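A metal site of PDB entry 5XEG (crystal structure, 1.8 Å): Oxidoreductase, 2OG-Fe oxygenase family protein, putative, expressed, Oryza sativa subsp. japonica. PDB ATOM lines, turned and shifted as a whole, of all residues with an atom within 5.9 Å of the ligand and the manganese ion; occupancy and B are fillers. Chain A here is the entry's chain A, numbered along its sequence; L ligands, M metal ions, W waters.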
ATOM      1  N   ARG A  48     -10.101  -7.056 -18.636  1.00  0.00           N
ATOM      2  CA  ARG A  48      -9.872  -7.320 -17.250  1.00  0.00           C
ATOM      3  C   ARG A  48      -8.400  -7.333 -17.003  1.00  0.00           C
ATOM      4  O   ARG A  48      -7.666  -7.897 -17.808  1.00  0.00           O
ATOM      5  CB  ARG A  48     -10.425  -8.693 -16.804  1.00  0.00           C
ATOM      6  CG  ARG A  48     -11.967  -8.784 -16.752  1.00  0.00           C
ATOM      7  CD  ARG A  48     -12.642  -7.880 -15.706  1.00  0.00           C
ATOM      8  NE  ARG A  48     -12.223  -8.266 -14.390  1.00  0.00           N
ATOM      9  CZ  ARG A  48     -12.862  -9.023 -13.509  1.00  0.00           C
ATOM     10  NH1 ARG A  48     -14.144  -9.366 -13.637  1.00  0.00           N
ATOM     11  NH2 ARG A  48     -12.215  -9.355 -12.424  1.00  0.00           N
ATOM     12  N   TRP A  64     -18.293  -1.187 -10.990  1.00  0.00           N
ATOM     13  CA  TRP A  64     -16.846  -1.187 -11.201  1.00  0.00           C
ATOM     14  C   TRP A  64     -16.581  -1.254 -12.723  1.00  0.00           C
ATOM     15  O   TRP A  64     -16.777  -2.298 -13.348  1.00  0.00           O
ATOM     16  CB  TRP A  64     -16.202  -2.382 -10.497  1.00  0.00           C
ATOM     17  CG  TRP A  64     -14.740  -2.523 -10.789  1.00  0.00           C
ATOM     18  CD1 TRP A  64     -13.745  -1.630 -10.502  1.00  0.00           C
ATOM     19  CD2 TRP A  64     -14.094  -3.630 -11.441  1.00  0.00           C
ATOM     20  NE1 TRP A  64     -12.533  -2.111 -10.922  1.00  0.00           N
ATOM     21  CE2 TRP A  64     -12.720  -3.334 -11.507  1.00  0.00           C
ATOM     22  CE3 TRP A  64     -14.556  -4.840 -11.972  1.00  0.00           C
ATOM     23  CZ2 TRP A  64     -11.793  -4.205 -12.079  1.00  0.00           C
ATOM     24  CZ3 TRP A  64     -13.639  -5.698 -12.545  1.00  0.00           C
ATOM     25  CH2 TRP A  64     -12.273  -5.385 -12.598  1.00  0.00           C
ATOM     26  N   LEU A 126     -18.769  -7.754  -6.973  1.00  0.00           N
ATOM     27  CA  LEU A 126     -18.562  -8.131  -8.343  1.00  0.00           C
ATOM     28  C   LEU A 126     -18.985  -9.606  -8.448  1.00  0.00           C
ATOM     29  O   LEU A 126     -18.479 -10.488  -7.709  1.00  0.00           O
ATOM     30  CB  LEU A 126     -17.108  -7.982  -8.664  1.00  0.00           C
ATOM     31  CG  LEU A 126     -16.607  -7.883 -10.081  1.00  0.00           C
ATOM     32  CD1 LEU A 126     -15.082  -7.839 -10.015  1.00  0.00           C
ATOM     33  CD2 LEU A 126     -17.120  -8.965 -11.002  1.00  0.00           C
ATOM     34  N   ASN A 128     -18.926 -12.611 -10.984  1.00  0.00           N
ATOM     35  CA  ASN A 128     -18.216 -13.181 -12.101  1.00  0.00           C
ATOM     36  C   ASN A 128     -18.838 -14.534 -12.424  1.00  0.00           C
ATOM     37  O   ASN A 128     -18.951 -15.404 -11.522  1.00  0.00           O
ATOM     38  CB  ASN A 128     -16.741 -13.420 -11.699  1.00  0.00           C
ATOM     39  CG  ASN A 128     -15.960 -12.165 -11.497  1.00  0.00           C
ATOM     40  OD1 ASN A 128     -15.813 -11.360 -12.436  1.00  0.00           O
ATOM     41  ND2 ASN A 128     -15.426 -11.971 -10.304  1.00  0.00           N
ATOM     42  N   TYR A 130     -18.014 -17.810 -14.825  1.00  0.00           N
ATOM     43  CA  TYR A 130     -17.103 -18.485 -15.715  1.00  0.00           C
ATOM     44  C   TYR A 130     -17.768 -19.724 -16.293  1.00  0.00           C
ATOM     45  O   TYR A 130     -18.327 -20.499 -15.513  1.00  0.00           O
ATOM     46  CB  TYR A 130     -15.911 -18.982 -14.911  1.00  0.00           C
ATOM     47  CG  TYR A 130     -15.097 -17.982 -14.167  1.00  0.00           C
ATOM     48  CD1 TYR A 130     -15.534 -17.500 -12.922  1.00  0.00           C
ATOM     49  CD2 TYR A 130     -13.862 -17.554 -14.649  1.00  0.00           C
ATOM     50  CE1 TYR A 130     -14.815 -16.573 -12.193  1.00  0.00           C
ATOM     51  CE2 TYR A 130     -13.133 -16.591 -13.923  1.00  0.00           C
ATOM     52  CZ  TYR A 130     -13.601 -16.176 -12.679  1.00  0.00           C
ATOM     53  OH  TYR A 130     -12.816 -15.256 -12.028  1.00  0.00           O
ATOM     54  N   LEU A 136      -9.070 -16.245 -15.299  1.00  0.00           N
ATOM     55  CA  LEU A 136      -8.871 -14.812 -14.944  1.00  0.00           C
ATOM     56  C   LEU A 136      -7.422 -14.690 -14.510  1.00  0.00           C
ATOM     57  O   LEU A 136      -7.021 -15.390 -13.583  1.00  0.00           O
ATOM     58  CB  LEU A 136      -9.794 -14.370 -13.827  1.00  0.00           C
ATOM     59  CG  LEU A 136      -9.697 -12.887 -13.418  1.00  0.00           C
ATOM     60  CD1 LEU A 136      -9.910 -11.922 -14.565  1.00  0.00           C
ATOM     61  CD2 LEU A 136     -10.596 -12.581 -12.236  1.00  0.00           C
ATOM     62  N   HIS A 139      -3.841 -10.608 -10.900  1.00  0.00           N
ATOM     63  CA  HIS A 139      -3.988  -9.170 -10.734  1.00  0.00           C
ATOM     64  C   HIS A 139      -4.128  -8.886  -9.245  1.00  0.00           C
ATOM     65  O   HIS A 139      -4.428  -9.806  -8.455  1.00  0.00           O
ATOM     66  CB  HIS A 139      -5.275  -8.630 -11.454  1.00  0.00           C
ATOM     67  CG  HIS A 139      -6.514  -9.222 -10.895  1.00  0.00           C
ATOM     68  ND1 HIS A 139      -6.880 -10.521 -11.165  1.00  0.00           N
ATOM     69  CD2 HIS A 139      -7.400  -8.760  -9.990  1.00  0.00           C
ATOM     70  CE1 HIS A 139      -7.958 -10.819 -10.464  1.00  0.00           C
ATOM     71  NE2 HIS A 139      -8.259  -9.783  -9.726  1.00  0.00           N
ATOM     72  N   GLN A 140      -4.000  -7.610  -8.891  1.00  0.00           N
ATOM     73  CA  GLN A 140      -4.285  -7.099  -7.551  1.00  0.00           C
ATOM     74  C   GLN A 140      -5.641  -6.394  -7.621  1.00  0.00           C
ATOM     75  O   GLN A 140      -5.931  -5.759  -8.600  1.00  0.00           O
ATOM     76  CB  GLN A 140      -3.236  -6.042  -7.195  1.00  0.00           C
ATOM     77  CG  GLN A 140      -1.869  -6.680  -6.928  1.00  0.00           C
ATOM     78  CD  GLN A 140      -0.806  -5.630  -6.603  1.00  0.00           C
ATOM     79  OE1 GLN A 140      -0.565  -4.675  -7.382  1.00  0.00           O
ATOM     80  NE2 GLN A 140      -0.144  -5.785  -5.444  1.00  0.00           N
ATOM     81  N   ASP A 141      -6.373  -6.411  -6.525  1.00  0.00           N
ATOM     82  CA  ASP A 141      -7.577  -5.597  -6.304  1.00  0.00           C
ATOM     83  C   ASP A 141      -7.055  -4.275  -5.774  1.00  0.00           C
ATOM     84  O   ASP A 141      -6.935  -4.042  -4.602  1.00  0.00           O
ATOM     85  CB  ASP A 141      -8.546  -6.263  -5.331  1.00  0.00           C
ATOM     86  CG  ASP A 141      -9.272  -7.479  -5.954  1.00  0.00           C
ATOM     87  OD1 ASP A 141      -9.009  -7.891  -7.104  1.00  0.00           O
ATOM     88  OD2 ASP A 141     -10.125  -7.991  -5.256  1.00  0.00           O
ATOM     89  N   SER A 157     -14.784 -13.381  -0.745  1.00  0.00           N
ATOM     90  CA  SER A 157     -15.129 -14.006  -2.023  1.00  0.00           C
ATOM     91  C   SER A 157     -15.922 -15.310  -1.796  1.00  0.00           C
ATOM     92  O   SER A 157     -15.428 -16.235  -1.118  1.00  0.00           O
ATOM     93  CB  SER A 157     -13.862 -14.354  -2.767  1.00  0.00           C
ATOM     94  OG  SER A 157     -14.020 -15.238  -3.890  1.00  0.00           O
ATOM     95  N   PHE A 158     -17.091 -15.370  -2.407  1.00  0.00           N
ATOM     96  CA  PHE A 158     -17.946 -16.539  -2.369  1.00  0.00           C
ATOM     97  C   PHE A 158     -17.654 -17.353  -3.639  1.00  0.00           C
ATOM     98  O   PHE A 158     -17.598 -16.788  -4.725  1.00  0.00           O
ATOM     99  CB  PHE A 158     -19.449 -16.251  -2.422  1.00  0.00           C
ATOM    100  CG  PHE A 158     -20.013 -15.430  -1.283  1.00  0.00           C
ATOM    101  CD1 PHE A 158     -19.281 -15.119  -0.167  1.00  0.00           C
ATOM    102  CD2 PHE A 158     -21.377 -15.135  -1.300  1.00  0.00           C
ATOM    103  CE1 PHE A 158     -19.838 -14.381   0.857  1.00  0.00           C
ATOM    104  CE2 PHE A 158     -21.968 -14.435  -0.245  1.00  0.00           C
ATOM    105  CZ  PHE A 158     -21.202 -14.072   0.837  1.00  0.00           C
ATOM    106  N   SER A 159     -17.679 -18.687  -3.497  1.00  0.00           N
ATOM    107  CA  SER A 159     -17.525 -19.582  -4.645  1.00  0.00           C
ATOM    108  C   SER A 159     -18.751 -20.519  -4.718  1.00  0.00           C
ATOM    109  O   SER A 159     -19.159 -21.117  -3.700  1.00  0.00           O
ATOM    110  CB  SER A 159     -16.262 -20.428  -4.537  1.00  0.00           C
ATOM    111  OG  SER A 159     -15.056 -19.656  -4.806  1.00  0.00           O
ATOM    112  N   ALA A 164     -12.853 -23.849  -8.699  1.00  0.00           N
ATOM    113  CA  ALA A 164     -11.782 -23.118  -9.375  1.00  0.00           C
ATOM    114  C   ALA A 164     -10.410 -23.472  -8.783  1.00  0.00           C
ATOM    115  O   ALA A 164     -10.299 -23.664  -7.568  1.00  0.00           O
ATOM    116  CB  ALA A 164     -11.995 -21.628  -9.185  1.00  0.00           C
ATOM    117  N   PHE A 166      -7.424 -21.565  -7.836  1.00  0.00           N
ATOM    118  CA  PHE A 166      -7.178 -20.153  -7.552  1.00  0.00           C
ATOM    119  C   PHE A 166      -5.708 -19.959  -7.258  1.00  0.00           C
ATOM    120  O   PHE A 166      -5.140 -20.636  -6.364  1.00  0.00           O
ATOM    121  CB  PHE A 166      -8.042 -19.760  -6.347  1.00  0.00           C
ATOM    122  CG  PHE A 166      -7.962 -18.341  -5.927  1.00  0.00           C
ATOM    123  CD1 PHE A 166      -8.709 -17.368  -6.594  1.00  0.00           C
ATOM    124  CD2 PHE A 166      -7.185 -17.961  -4.836  1.00  0.00           C
ATOM    125  CE1 PHE A 166      -8.660 -16.038  -6.176  1.00  0.00           C
ATOM    126  CE2 PHE A 166      -7.131 -16.637  -4.448  1.00  0.00           C
ATOM    127  CZ  PHE A 166      -7.888 -15.705  -5.066  1.00  0.00           C
ATOM    128  N   LEU A 182     -10.912 -23.636  -4.779  1.00  0.00           N
ATOM    129  CA  LEU A 182     -12.110 -23.018  -4.239  1.00  0.00           C
ATOM    130  C   LEU A 182     -13.255 -23.803  -4.751  1.00  0.00           C
ATOM    131  O   LEU A 182     -13.537 -23.820  -5.956  1.00  0.00           O
ATOM    132  CB  LEU A 182     -12.192 -21.560  -4.640  1.00  0.00           C
ATOM    133  CG  LEU A 182     -10.983 -20.715  -4.163  1.00  0.00           C
ATOM    134  CD1 LEU A 182     -11.168 -19.263  -4.667  1.00  0.00           C
ATOM    135  CD2 LEU A 182     -10.865 -20.691  -2.667  1.00  0.00           C
ATOM    136  N   PHE A 190      -9.220 -12.203   2.011  1.00  0.00           N
ATOM    137  CA  PHE A 190      -7.893 -11.671   2.070  1.00  0.00           C
ATOM    138  C   PHE A 190      -7.963 -10.201   2.457  1.00  0.00           C
ATOM    139  O   PHE A 190      -8.588  -9.369   1.783  1.00  0.00           O
ATOM    140  CB  PHE A 190      -7.041 -11.932   0.806  1.00  0.00           C
ATOM    141  CG  PHE A 190      -7.676 -11.609  -0.516  1.00  0.00           C
ATOM    142  CD1 PHE A 190      -8.492 -12.546  -1.171  1.00  0.00           C
ATOM    143  CD2 PHE A 190      -7.316 -10.480  -1.257  1.00  0.00           C
ATOM    144  CE1 PHE A 190      -9.030 -12.318  -2.418  1.00  0.00           C
ATOM    145  CE2 PHE A 190      -7.808 -10.280  -2.581  1.00  0.00           C
ATOM    146  CZ  PHE A 190      -8.701 -11.187  -3.116  1.00  0.00           C
ATOM    147  N   HIS A 199      -3.641 -12.410  -7.634  1.00  0.00           N
ATOM    148  CA  HIS A 199      -4.506 -13.569  -7.552  1.00  0.00           C
ATOM    149  C   HIS A 199      -5.266 -13.719  -8.849  1.00  0.00           C
ATOM    150  O   HIS A 199      -5.343 -12.785  -9.683  1.00  0.00           O
ATOM    151  CB  HIS A 199      -5.474 -13.519  -6.363  1.00  0.00           C
ATOM    152  CG  HIS A 199      -6.366 -12.340  -6.397  1.00  0.00           C
ATOM    153  ND1 HIS A 199      -5.928 -11.073  -6.030  1.00  0.00           N
ATOM    154  CD2 HIS A 199      -7.626 -12.189  -6.853  1.00  0.00           C
ATOM    155  CE1 HIS A 199      -6.898 -10.208  -6.248  1.00  0.00           C
ATOM    156  NE2 HIS A 199      -7.955 -10.861  -6.682  1.00  0.00           N
ATOM    157  N   GLY A 200      -5.754 -14.932  -9.063  1.00  0.00           N
ATOM    158  CA  GLY A 200      -6.516 -15.157 -10.275  1.00  0.00           C
ATOM    159  C   GLY A 200      -7.022 -16.612 -10.338  1.00  0.00           C
ATOM    160  O   GLY A 200      -6.851 -17.356  -9.391  1.00  0.00           O
ATOM    161  N   VAL A 201      -7.679 -16.966 -11.438  1.00  0.00           N
ATOM    162  CA  VAL A 201      -8.318 -18.276 -11.597  1.00  0.00           C
ATOM    163  C   VAL A 201      -7.643 -18.933 -12.835  1.00  0.00           C
ATOM    164  O   VAL A 201      -7.774 -18.427 -13.942  1.00  0.00           O
ATOM    165  CB  VAL A 201      -9.845 -18.140 -11.765  1.00  0.00           C
ATOM    166  CG1 VAL A 201     -10.435 -19.512 -12.082  1.00  0.00           C
ATOM    167  CG2 VAL A 201     -10.475 -17.616 -10.512  1.00  0.00           C
ATOM    168  N   ARG A 223     -18.919 -21.815 -12.997  1.00  0.00           N
ATOM    169  CA  ARG A 223     -18.698 -21.345 -11.635  1.00  0.00           C
ATOM    170  C   ARG A 223     -19.182 -19.903 -11.466  1.00  0.00           C
ATOM    171  O   ARG A 223     -18.928 -19.070 -12.338  1.00  0.00           O
ATOM    172  CB  ARG A 223     -17.226 -21.372 -11.289  1.00  0.00           C
ATOM    173  CG  ARG A 223     -16.897 -20.790  -9.938  1.00  0.00           C
ATOM    174  CD  ARG A 223     -15.429 -21.012  -9.619  1.00  0.00           C
ATOM    175  NE  ARG A 223     -15.017 -20.283  -8.409  1.00  0.00           N
ATOM    176  CZ  ARG A 223     -14.452 -19.060  -8.362  1.00  0.00           C
ATOM    177  NH1 ARG A 223     -14.183 -18.341  -9.454  1.00  0.00           N
ATOM    178  NH2 ARG A 223     -14.140 -18.541  -7.193  1.00  0.00           N
ATOM    179  N   ASN A 225     -18.810 -16.680  -8.968  1.00  0.00           N
ATOM    180  CA  ASN A 225     -18.068 -16.074  -7.893  1.00  0.00           C
ATOM    181  C   ASN A 225     -18.731 -14.748  -7.557  1.00  0.00           C
ATOM    182  O   ASN A 225     -19.199 -14.054  -8.461  1.00  0.00           O
ATOM    183  CB  ASN A 225     -16.621 -15.809  -8.344  1.00  0.00           C
ATOM    184  CG  ASN A 225     -15.902 -14.798  -7.465  1.00  0.00           C
ATOM    185  OD1 ASN A 225     -15.746 -13.635  -7.815  1.00  0.00           O
ATOM    186  ND2 ASN A 225     -15.491 -15.238  -6.290  1.00  0.00           N
ATOM    187  N   THR A 227     -17.527 -11.364  -5.372  1.00  0.00           N
ATOM    188  CA  THR A 227     -16.389 -10.784  -4.700  1.00  0.00           C
ATOM    189  C   THR A 227     -16.844  -9.440  -4.107  1.00  0.00           C
ATOM    190  O   THR A 227     -17.252  -8.572  -4.864  1.00  0.00           O
ATOM    191  CB  THR A 227     -15.222 -10.606  -5.666  1.00  0.00           C
ATOM    192  OG1 THR A 227     -14.746 -11.932  -5.963  1.00  0.00           O
ATOM    193  CG2 THR A 227     -14.125  -9.809  -4.991  1.00  0.00           C
ATOM    194  N   ARG A 229     -16.183  -5.995  -1.683  1.00  0.00           N
ATOM    195  CA  ARG A 229     -15.169  -5.062  -1.254  1.00  0.00           C
ATOM    196  C   ARG A 229     -15.822  -3.759  -0.729  1.00  0.00           C
ATOM    197  O   ARG A 229     -17.011  -3.569  -0.935  1.00  0.00           O
ATOM    198  CB  ARG A 229     -14.254  -4.707  -2.439  1.00  0.00           C
ATOM    199  CG  ARG A 229     -13.632  -5.937  -3.115  1.00  0.00           C
ATOM    200  CD  ARG A 229     -12.451  -5.618  -4.006  1.00  0.00           C
ATOM    201  NE  ARG A 229     -12.901  -5.106  -5.271  1.00  0.00           N
ATOM    202  CZ  ARG A 229     -12.919  -5.749  -6.450  1.00  0.00           C
ATOM    203  NH1 ARG A 229     -12.502  -6.982  -6.639  1.00  0.00           N
ATOM    204  NH2 ARG A 229     -13.393  -5.083  -7.479  1.00  0.00           N
HETATM  205  C1  LIG L   1     -12.003 -10.580  -9.333  1.00  0.00           C
HETATM  206  O1  LIG L   1     -11.482  -9.504  -8.961  1.00  0.00           O
HETATM  207  O2  LIG L   1     -12.924 -10.613 -10.172  1.00  0.00           O
HETATM  208  C2  LIG L   1     -11.504 -11.838  -8.784  1.00  0.00           C
HETATM  209  O3  LIG L   1     -10.340 -11.941  -8.446  1.00  0.00           O
HETATM  210  C3  LIG L   1     -12.445 -13.013  -8.624  1.00  0.00           C
HETATM  211  C4  LIG L   1     -11.640 -14.301  -8.569  1.00  0.00           C
HETATM  212  C5  LIG L   1     -12.586 -15.477  -8.481  1.00  0.00           C
HETATM  213  O4  LIG L   1     -12.525 -16.220  -7.474  1.00  0.00           O
HETATM  214  O5  LIG L   1     -13.392 -15.670  -9.410  1.00  0.00           O
HETATM  215 MN    MN M   1      -9.561  -9.871  -7.842  1.00  0.00          MN
HETATM  216  O   HOH W   1     -11.996 -12.467  -5.333  1.00  0.00           O
HETATM  217  O   HOH W   2     -12.132  -6.734  -9.560  1.00  0.00           O
HETATM  218  O   HOH W   3     -11.807 -15.472  -5.087  1.00  0.00           O
HETATM  219  O   HOH W   4     -10.922 -10.200  -6.149  1.00  0.00           O
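NH2 of Arg 48 is in salt-bridge range of O2 of the ligand, at 2.7 Å.
The side-chain hydroxyl of Tyr 130 lies within hydrogen-bond range of an oxygen (O5) of the ligand (2.7 Å).
The guanidinium group (NH1) of Arg 223 is in salt-bridge range of an oxygen (O5) of the ligand (2.8 Å).
The side-chain amide nitrogen of Asn 128 lies within hydrogen-bond range of an oxygen (O2) of the ligand (2.8 Å).
O4 of the ligand is in hydrogen-bond range of ND2 of Asn 225 (3.3 Å).
The guanidinium group of Arg 229 sits close to an oxygen (O1) of the ligand (3.6 Å).
The side-chain carboxylate (OD2) of Asp 141 is in salt-bridge range of the guanidinium group (NH1) of Arg 229 (2.9 Å).
The side-chain amide oxygen of Asn 128 sits at hydrogen-bond distance from the guanidinium group of Arg 48, at 2.9 Å.
The guanidinium group (NH2) of Arg 223 sits at hydrogen-bond distance from the side-chain hydroxyl (OG) of Ser 159 (2.8 Å).
The backbone NH (N) of Asn 225 lies within hydrogen-bond range of the backbone carbonyl oxygen (O) of Asn 128, 2.9 Å away.
The side-chain amide oxygen (OD1) of Asn 225 is in hydrogen-bond range of the side-chain hydroxyl (OG1) of Thr 227 (2.7 Å).
ND2 of Asn 225 sits at hydrogen-bond distance from OG of Ser 157 (2.8 Å).
The backbone carbonyl oxygen (O) of Phe 158 sits at hydrogen-bond distance from the side-chain amide nitrogen (ND2) of Asn 225.
The backbone NH of Val 201 sits at hydrogen-bond distance from the backbone carbonyl oxygen of Leu 136 (2.7 Å).
Water W3 bridges the side-chain hydroxyl of Ser 157 and an oxygen (O4) of the ligand.
The manganese ion is bound by OD1 of Asp 141, water W4, NE2 of His 199, O1 of the ligand, NE2 of His 139 and O3 of the ligand.
The manganese ion has six donor atoms within binding distance.
Merely in contact with the ligand: Leu 126, Leu 136, Val 201 and Thr 227.
Hydrophobic or aromatic side chains within 4 Å of the ligand: Leu 126, Tyr 130, Leu 136, His 139, His 199 and Val 201.
Of the 23 residues printed, 13 come within 4 Å of the ligand.
Within 4 Å of the manganese ion: His 139, Asp 141 and His 199.
The nearest printed residue that does not touch the manganese ion is Arg 229 (4.3 Å).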
